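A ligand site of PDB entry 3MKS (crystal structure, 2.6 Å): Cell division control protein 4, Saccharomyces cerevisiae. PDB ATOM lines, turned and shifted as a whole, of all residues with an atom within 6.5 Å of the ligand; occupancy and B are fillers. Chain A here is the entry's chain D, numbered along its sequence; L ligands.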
ATOM      1  N   THR A 332     -10.646 -20.393   7.411  1.00  0.00           N
ATOM      2  CA  THR A 332      -9.219 -20.128   7.525  1.00  0.00           C
ATOM      3  C   THR A 332      -8.753 -19.773   8.944  1.00  0.00           C
ATOM      4  O   THR A 332      -7.636 -19.316   9.142  1.00  0.00           O
ATOM      5  CB  THR A 332      -8.907 -18.980   6.498  1.00  0.00           C
ATOM      6  OG1 THR A 332      -8.233 -19.549   5.376  1.00  0.00           O
ATOM      7  CG2 THR A 332      -8.150 -17.799   7.055  1.00  0.00           C
ATOM      8  N   ILE A 334      -8.717 -20.748  13.330  1.00  0.00           N
ATOM      9  CA  ILE A 334      -8.996 -21.634  14.419  1.00  0.00           C
ATOM     10  C   ILE A 334      -9.561 -20.784  15.532  1.00  0.00           C
ATOM     11  O   ILE A 334      -9.090 -19.643  15.801  1.00  0.00           O
ATOM     12  CB  ILE A 334      -7.747 -22.314  14.897  1.00  0.00           C
ATOM     13  CG1 ILE A 334      -7.369 -23.438  13.911  1.00  0.00           C
ATOM     14  CG2 ILE A 334      -7.978 -22.832  16.280  1.00  0.00           C
ATOM     15  CD1 ILE A 334      -5.929 -24.001  14.063  1.00  0.00           C
ATOM     16  N   LEU A 348      -7.283 -17.679  16.003  1.00  0.00           N
ATOM     17  CA  LEU A 348      -5.938 -17.848  15.410  1.00  0.00           C
ATOM     18  C   LEU A 348      -6.009 -17.747  13.903  1.00  0.00           C
ATOM     19  O   LEU A 348      -6.869 -18.397  13.284  1.00  0.00           O
ATOM     20  CB  LEU A 348      -5.359 -19.205  15.794  1.00  0.00           C
ATOM     21  CG  LEU A 348      -5.357 -19.598  17.279  1.00  0.00           C
ATOM     22  CD1 LEU A 348      -4.561 -20.893  17.502  1.00  0.00           C
ATOM     23  CD2 LEU A 348      -4.757 -18.496  18.181  1.00  0.00           C
ATOM     24  N   GLN A 349      -5.076 -16.983  13.304  1.00  0.00           N
ATOM     25  CA  GLN A 349      -5.069 -16.678  11.875  1.00  0.00           C
ATOM     26  C   GLN A 349      -3.808 -15.942  11.493  1.00  0.00           C
ATOM     27  O   GLN A 349      -3.299 -15.109  12.266  1.00  0.00           O
ATOM     28  CB  GLN A 349      -6.231 -15.784  11.592  1.00  0.00           C
ATOM     29  CG  GLN A 349      -6.692 -15.682  10.126  1.00  0.00           C
ATOM     30  CD  GLN A 349      -7.841 -14.719   9.968  1.00  0.00           C
ATOM     31  OE1 GLN A 349      -8.552 -14.786   8.977  1.00  0.00           O
ATOM     32  NE2 GLN A 349      -8.047 -13.838  10.963  1.00  0.00           N
ATOM     33  N   GLY A 350      -3.295 -16.116  10.285  1.00  0.00           N
ATOM     34  CA  GLY A 350      -4.046 -16.496   9.124  1.00  0.00           C
ATOM     35  C   GLY A 350      -3.086 -16.089   8.048  1.00  0.00           C
ATOM     36  O   GLY A 350      -1.920 -16.015   8.335  1.00  0.00           O
ATOM     37  N   HIS A 351      -3.515 -15.850   6.821  1.00  0.00           N
ATOM     38  CA  HIS A 351      -2.554 -15.857   5.692  1.00  0.00           C
ATOM     39  C   HIS A 351      -2.535 -17.041   4.765  1.00  0.00           C
ATOM     40  O   HIS A 351      -2.208 -16.862   3.623  1.00  0.00           O
ATOM     41  CB  HIS A 351      -1.101 -15.616   6.126  1.00  0.00           C
ATOM     42  CG  HIS A 351      -0.733 -14.173   6.054  1.00  0.00           C
ATOM     43  ND1 HIS A 351      -1.399 -13.274   5.248  1.00  0.00           N
ATOM     44  CD2 HIS A 351       0.224 -13.464   6.698  1.00  0.00           C
ATOM     45  CE1 HIS A 351      -0.871 -12.070   5.400  1.00  0.00           C
ATOM     46  NE2 HIS A 351       0.108 -12.160   6.283  1.00  0.00           N
ATOM     47  N   THR A 352      -2.826 -18.243   5.244  1.00  0.00           N
ATOM     48  CA  THR A 352      -2.936 -19.392   4.368  1.00  0.00           C
ATOM     49  C   THR A 352      -3.974 -20.184   5.131  1.00  0.00           C
ATOM     50  O   THR A 352      -4.023 -20.060   6.345  1.00  0.00           O
ATOM     51  CB  THR A 352      -1.552 -20.121   4.279  1.00  0.00           C
ATOM     52  OG1 THR A 352      -0.719 -19.384   3.375  1.00  0.00           O
ATOM     53  CG2 THR A 352      -1.645 -21.552   3.778  1.00  0.00           C
ATOM     54  N   ALA A 353      -4.835 -20.918   4.399  1.00  0.00           N
ATOM     55  CA  ALA A 353      -5.855 -21.810   5.014  1.00  0.00           C
ATOM     56  C   ALA A 353      -5.220 -22.930   5.904  1.00  0.00           C
ATOM     57  O   ALA A 353      -4.078 -23.345   5.658  1.00  0.00           O
ATOM     58  CB  ALA A 353      -6.756 -22.448   3.929  1.00  0.00           C
ATOM     59  N   LEU A 354      -5.949 -23.365   6.928  1.00  0.00           N
ATOM     60  CA  LEU A 354      -5.656 -24.623   7.613  1.00  0.00           C
ATOM     61  C   LEU A 354      -6.269 -25.806   6.837  1.00  0.00           C
ATOM     62  O   LEU A 354      -7.261 -25.664   6.112  1.00  0.00           O
ATOM     63  CB  LEU A 354      -6.159 -24.593   9.059  1.00  0.00           C
ATOM     64  CG  LEU A 354      -5.422 -23.770  10.149  1.00  0.00           C
ATOM     65  CD1 LEU A 354      -3.842 -23.896  10.179  1.00  0.00           C
ATOM     66  CD2 LEU A 354      -5.838 -22.258  10.170  1.00  0.00           C
ATOM     67  N   ALA A 368      -2.108 -28.792  10.378  1.00  0.00           N
ATOM     68  CA  ALA A 368      -1.524 -28.560   9.079  1.00  0.00           C
ATOM     69  C   ALA A 368      -2.165 -27.321   8.442  1.00  0.00           C
ATOM     70  O   ALA A 368      -3.300 -26.904   8.817  1.00  0.00           O
ATOM     71  CB  ALA A 368      -1.646 -29.775   8.153  1.00  0.00           C
ATOM     72  N   ALA A 369      -1.416 -26.785   7.469  1.00  0.00           N
ATOM     73  CA  ALA A 369      -1.769 -25.591   6.686  1.00  0.00           C
ATOM     74  C   ALA A 369      -1.545 -25.798   5.150  1.00  0.00           C
ATOM     75  O   ALA A 369      -0.800 -26.681   4.707  1.00  0.00           O
ATOM     76  CB  ALA A 369      -0.949 -24.329   7.203  1.00  0.00           C
ATOM     77  N   ALA A 370      -2.211 -24.962   4.353  1.00  0.00           N
ATOM     78  CA  ALA A 370      -2.412 -25.162   2.905  1.00  0.00           C
ATOM     79  C   ALA A 370      -1.153 -24.790   2.175  1.00  0.00           C
ATOM     80  O   ALA A 370      -1.218 -24.521   0.985  1.00  0.00           O
ATOM     81  CB  ALA A 370      -3.511 -24.287   2.422  1.00  0.00           C
ATOM     82  N   ASP A 371      -0.023 -24.767   2.878  1.00  0.00           N
ATOM     83  CA  ASP A 371       1.214 -24.355   2.250  1.00  0.00           C
ATOM     84  C   ASP A 371       2.336 -25.336   2.503  1.00  0.00           C
ATOM     85  O   ASP A 371       3.500 -25.006   2.331  1.00  0.00           O
ATOM     86  CB  ASP A 371       1.601 -22.917   2.653  1.00  0.00           C
ATOM     87  CG  ASP A 371       1.983 -22.761   4.137  1.00  0.00           C
ATOM     88  OD1 ASP A 371       1.643 -23.617   5.017  1.00  0.00           O
ATOM     89  OD2 ASP A 371       2.623 -21.744   4.446  1.00  0.00           O
ATOM     90  N   SER A 373       2.891 -26.920   5.437  1.00  0.00           N
ATOM     91  CA  SER A 373       3.479 -26.796   6.752  1.00  0.00           C
ATOM     92  C   SER A 373       2.610 -27.432   7.790  1.00  0.00           C
ATOM     93  O   SER A 373       1.385 -27.594   7.584  1.00  0.00           O
ATOM     94  CB  SER A 373       3.628 -25.319   7.089  1.00  0.00           C
ATOM     95  OG  SER A 373       2.360 -24.674   7.187  1.00  0.00           O
ATOM     96  N   ILE A 374       3.242 -27.758   8.914  1.00  0.00           N
ATOM     97  CA  ILE A 374       2.560 -27.954  10.175  1.00  0.00           C
ATOM     98  C   ILE A 374       2.920 -26.860  11.190  1.00  0.00           C
ATOM     99  O   ILE A 374       4.083 -26.479  11.320  1.00  0.00           O
ATOM    100  CB  ILE A 374       2.893 -29.333  10.794  1.00  0.00           C
ATOM    101  CG1 ILE A 374       2.601 -30.413   9.764  1.00  0.00           C
ATOM    102  CG2 ILE A 374       2.013 -29.577  12.018  1.00  0.00           C
ATOM    103  CD1 ILE A 374       3.774 -30.790   9.001  1.00  0.00           C
ATOM    104  N   ARG A 375       1.915 -26.370  11.885  1.00  0.00           N
ATOM    105  CA  ARG A 375       2.043 -25.334  12.864  1.00  0.00           C
ATOM    106  C   ARG A 375       1.684 -25.827  14.263  1.00  0.00           C
ATOM    107  O   ARG A 375       0.714 -26.599  14.427  1.00  0.00           O
ATOM    108  CB  ARG A 375       1.080 -24.231  12.510  1.00  0.00           C
ATOM    109  CG  ARG A 375       1.242 -23.684  11.110  1.00  0.00           C
ATOM    110  CD  ARG A 375       2.620 -23.123  10.886  1.00  0.00           C
ATOM    111  NE  ARG A 375       2.692 -22.617   9.538  1.00  0.00           N
ATOM    112  CZ  ARG A 375       3.348 -21.526   9.165  1.00  0.00           C
ATOM    113  NH1 ARG A 375       4.028 -20.790  10.052  1.00  0.00           N
ATOM    114  NH2 ARG A 375       3.265 -21.161   7.886  1.00  0.00           N
ATOM    115  N   GLY A 376       2.446 -25.391  15.263  1.00  0.00           N
ATOM    116  CA  GLY A 376       2.145 -25.704  16.630  1.00  0.00           C
ATOM    117  C   GLY A 376       2.100 -24.476  17.482  1.00  0.00           C
ATOM    118  O   GLY A 376       2.958 -23.576  17.369  1.00  0.00           O
ATOM    119  N   TRP A 377       1.070 -24.462  18.312  1.00  0.00           N
ATOM    120  CA  TRP A 377       0.784 -23.468  19.321  1.00  0.00           C
ATOM    121  C   TRP A 377       0.794 -24.148  20.702  1.00  0.00           C
ATOM    122  O   TRP A 377       0.493 -25.319  20.834  1.00  0.00           O
ATOM    123  CB  TRP A 377      -0.632 -22.943  19.104  1.00  0.00           C
ATOM    124  CG  TRP A 377      -0.858 -22.163  17.875  1.00  0.00           C
ATOM    125  CD1 TRP A 377      -0.672 -20.779  17.692  1.00  0.00           C
ATOM    126  CD2 TRP A 377      -1.321 -22.665  16.629  1.00  0.00           C
ATOM    127  NE1 TRP A 377      -1.013 -20.442  16.392  1.00  0.00           N
ATOM    128  CE2 TRP A 377      -1.404 -21.575  15.733  1.00  0.00           C
ATOM    129  CE3 TRP A 377      -1.627 -23.944  16.175  1.00  0.00           C
ATOM    130  CZ2 TRP A 377      -1.787 -21.747  14.423  1.00  0.00           C
ATOM    131  CZ3 TRP A 377      -2.022 -24.096  14.867  1.00  0.00           C
ATOM    132  CH2 TRP A 377      -2.110 -23.002  14.017  1.00  0.00           C
ATOM    133  N   TYR A 382      -1.763 -20.825  23.630  1.00  0.00           N
ATOM    134  CA  TYR A 382      -1.765 -20.670  22.154  1.00  0.00           C
ATOM    135  C   TYR A 382      -0.770 -19.666  21.628  1.00  0.00           C
ATOM    136  O   TYR A 382      -1.006 -19.133  20.551  1.00  0.00           O
ATOM    137  CB  TYR A 382      -3.157 -20.313  21.593  1.00  0.00           C
ATOM    138  CG  TYR A 382      -4.165 -21.172  22.263  1.00  0.00           C
ATOM    139  CD1 TYR A 382      -4.843 -20.706  23.372  1.00  0.00           C
ATOM    140  CD2 TYR A 382      -4.344 -22.487  21.882  1.00  0.00           C
ATOM    141  CE1 TYR A 382      -5.678 -21.520  24.061  1.00  0.00           C
ATOM    142  CE2 TYR A 382      -5.198 -23.299  22.558  1.00  0.00           C
ATOM    143  CZ  TYR A 382      -5.865 -22.807  23.671  1.00  0.00           C
ATOM    144  OH  TYR A 382      -6.754 -23.613  24.395  1.00  0.00           O
ATOM    145  N   SER A 383       0.338 -19.429  22.335  1.00  0.00           N
ATOM    146  CA  SER A 383       1.460 -18.722  21.670  1.00  0.00           C
ATOM    147  C   SER A 383       2.103 -19.610  20.607  1.00  0.00           C
ATOM    148  O   SER A 383       1.896 -20.847  20.568  1.00  0.00           O
ATOM    149  CB  SER A 383       2.497 -18.182  22.644  1.00  0.00           C
ATOM    150  OG  SER A 383       2.857 -19.198  23.494  1.00  0.00           O
ATOM    151  N   ARG A 384       2.786 -18.956  19.681  1.00  0.00           N
ATOM    152  CA  ARG A 384       3.399 -19.637  18.542  1.00  0.00           C
ATOM    153  C   ARG A 384       4.579 -20.479  19.054  1.00  0.00           C
ATOM    154  O   ARG A 384       5.405 -19.976  19.843  1.00  0.00           O
ATOM    155  CB  ARG A 384       3.897 -18.583  17.563  1.00  0.00           C
ATOM    156  CG  ARG A 384       2.929 -17.953  16.613  1.00  0.00           C
ATOM    157  CD  ARG A 384       3.697 -16.903  15.842  1.00  0.00           C
ATOM    158  NE  ARG A 384       2.866 -16.275  14.805  1.00  0.00           N
ATOM    159  CZ  ARG A 384       3.195 -15.186  14.096  1.00  0.00           C
ATOM    160  NH1 ARG A 384       4.375 -14.552  14.278  1.00  0.00           N
ATOM    161  NH2 ARG A 384       2.342 -14.740  13.156  1.00  0.00           N
ATOM    162  N   LYS A 385       4.637 -21.759  18.641  1.00  0.00           N
ATOM    163  CA  LYS A 385       5.684 -22.674  19.117  1.00  0.00           C
ATOM    164  C   LYS A 385       6.555 -23.277  18.018  1.00  0.00           C
ATOM    165  O   LYS A 385       7.729 -23.455  18.234  1.00  0.00           O
ATOM    166  CB  LYS A 385       5.092 -23.797  19.976  1.00  0.00           C
ATOM    167  CG  LYS A 385       4.728 -23.457  21.441  1.00  0.00           C
ATOM    168  CD  LYS A 385       5.936 -22.990  22.251  1.00  0.00           C
ATOM    169  CE  LYS A 385       5.496 -22.340  23.569  1.00  0.00           C
ATOM    170  NZ  LYS A 385       6.655 -22.429  24.494  1.00  0.00           N
ATOM    171  N   PHE A 386       5.981 -23.666  16.874  1.00  0.00           N
ATOM    172  CA  PHE A 386       6.791 -24.234  15.800  1.00  0.00           C
ATOM    173  C   PHE A 386       6.149 -24.166  14.419  1.00  0.00           C
ATOM    174  O   PHE A 386       4.922 -24.170  14.289  1.00  0.00           O
ATOM    175  CB  PHE A 386       7.253 -25.672  16.111  1.00  0.00           C
ATOM    176  CG  PHE A 386       6.146 -26.701  16.249  1.00  0.00           C
ATOM    177  CD1 PHE A 386       5.366 -27.090  15.180  1.00  0.00           C
ATOM    178  CD2 PHE A 386       5.907 -27.322  17.467  1.00  0.00           C
ATOM    179  CE1 PHE A 386       4.347 -28.070  15.324  1.00  0.00           C
ATOM    180  CE2 PHE A 386       4.909 -28.278  17.599  1.00  0.00           C
ATOM    181  CZ  PHE A 386       4.140 -28.641  16.533  1.00  0.00           C
ATOM    182  N   SER A 387       6.971 -24.079  13.387  1.00  0.00           N
ATOM    183  CA  SER A 387       6.518 -24.338  12.014  1.00  0.00           C
ATOM    184  C   SER A 387       7.483 -25.185  11.303  1.00  0.00           C
ATOM    185  O   SER A 387       8.688 -24.936  11.333  1.00  0.00           O
ATOM    186  CB  SER A 387       6.416 -23.054  11.214  1.00  0.00           C
ATOM    187  OG  SER A 387       5.780 -22.137  12.042  1.00  0.00           O
HETATM  188  C1  LIG L   1       3.546 -21.164  14.638  1.00  0.00           C
HETATM  189  C2  LIG L   1       4.248 -20.167  13.988  1.00  0.00           C
HETATM  190  C3  LIG L   1       3.564 -19.300  13.136  1.00  0.00           C
HETATM  191  C4  LIG L   1       2.145 -19.416  12.970  1.00  0.00           C
HETATM  192  C5  LIG L   1       1.457 -20.426  13.668  1.00  0.00           C
HETATM  193  C6  LIG L   1       2.157 -21.300  14.483  1.00  0.00           C
HETATM  194  C7  LIG L   1       4.287 -18.296  12.488  1.00  0.00           C
HETATM  195  C8  LIG L   1       3.572 -17.429  11.663  1.00  0.00           C
HETATM  196  C9  LIG L   1       2.183 -17.549  11.494  1.00  0.00           C
HETATM  197  C10 LIG L   1       1.429 -18.535  12.154  1.00  0.00           C
HETATM  198  C11 LIG L   1       0.039 -18.706  12.029  1.00  0.00           C
HETATM  199  C12 LIG L   1      -0.485 -19.379  10.911  1.00  0.00           C
HETATM  200  C13 LIG L   1      -1.838 -19.612  10.797  1.00  0.00           C
HETATM  201  C14 LIG L   1      -2.709 -19.200  11.786  1.00  0.00           C
HETATM  202  C15 LIG L   1      -2.225 -18.550  12.903  1.00  0.00           C
HETATM  203  C16 LIG L   1      -0.859 -18.300  13.024  1.00  0.00           C
HETATM  204  C17 LIG L   1       0.358 -19.830   9.895  1.00  0.00           C
HETATM  205  C18 LIG L   1      -0.156 -20.476   8.781  1.00  0.00           C
HETATM  206  C19 LIG L   1      -1.532 -20.707   8.661  1.00  0.00           C
HETATM  207  C20 LIG L   1      -2.354 -20.280   9.684  1.00  0.00           C
HETATM  208  C21 LIG L   1      -0.446 -17.606  14.295  1.00  0.00           C
HETATM  209  O1  LIG L   1      -0.929 -18.092  15.380  1.00  0.00           O
HETATM  210  O2  LIG L   1       0.376 -16.671  14.188  1.00  0.00           O
HETATM  211  C22 LIG L   1       1.502 -16.564  10.603  1.00  0.00           C
HETATM  212  O3  LIG L   1       0.624 -15.877  11.126  1.00  0.00           O
HETATM  213  O4  LIG L   1       1.882 -16.455   9.434  1.00  0.00           O
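C of Leu 348 touches C15 of the ligand, 3.995 Å away.
Gln 349 touches the ligand (N to C15, 3.3 Å).
N of Gly 350 touches C14 of the ligand (3.5 Å).
O of Thr 352 touches C19 of the ligand, at 3.5 Å.
Leu 354 touches the ligand.
Ala 369 touches the ligand (CB to C19, 3.9 Å).
NH1 of Arg 375 touches C3 of the ligand (3.5 Å).
Gly 376 touches the ligand.
Phe 386 touches the ligand (O to C1, 3.3 Å).
Ser 387 touches the ligand (OG to C2, 3.2 Å).
Hydrophobic or aromatic side chains that line the ligand: Leu 354, Ala 369 and Trp 377.
Within 4 Å of the ligand: Leu 348, Gln 349, Gly 350, Thr 352, Leu 354, Ala 369, Arg 375, Gly 376, Trp 377, Arg 384, Phe 386 and Ser 387.
The nearest printed residue that does not touch the ligand is Lys 385 (4.2 Å).
The side-chain hydroxyl (OG) of Ser 387 sits at hydrogen-bond distance from the guanidinium group (NH1) of Arg 375 (3.0 Å).
The backbone carbonyl oxygen of Phe 386 is in hydrogen-bond range of the backbone NH of Gly 376 (2.9 Å).
The guanidinium group (NE) of Arg 375 is in hydrogen-bond range of the side-chain hydroxyl (OG) of Ser 373 (3.1 Å).
The guanidinium group (NH2) of Arg 375 lies within salt-bridge range of the side-chain carboxylate (OD2) of Asp 371 (3.5 Å).
The backbone carbonyl oxygen (O) of Gly 376 is in hydrogen-bond range of the backbone NH (N) of Lys 385 (2.8 Å).
The backbone NH (N) of Leu 348 sits at hydrogen-bond distance from the backbone carbonyl oxygen (O) of Ile 334 (2.7 Å).
The indole nitrogen (NE1) of Trp 377 is in hydrogen-bond range of an oxygen (O1) of the ligand (2.6 Å).
NE of Arg 384 is in salt-bridge range of O2 of the ligand (2.6 Å).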
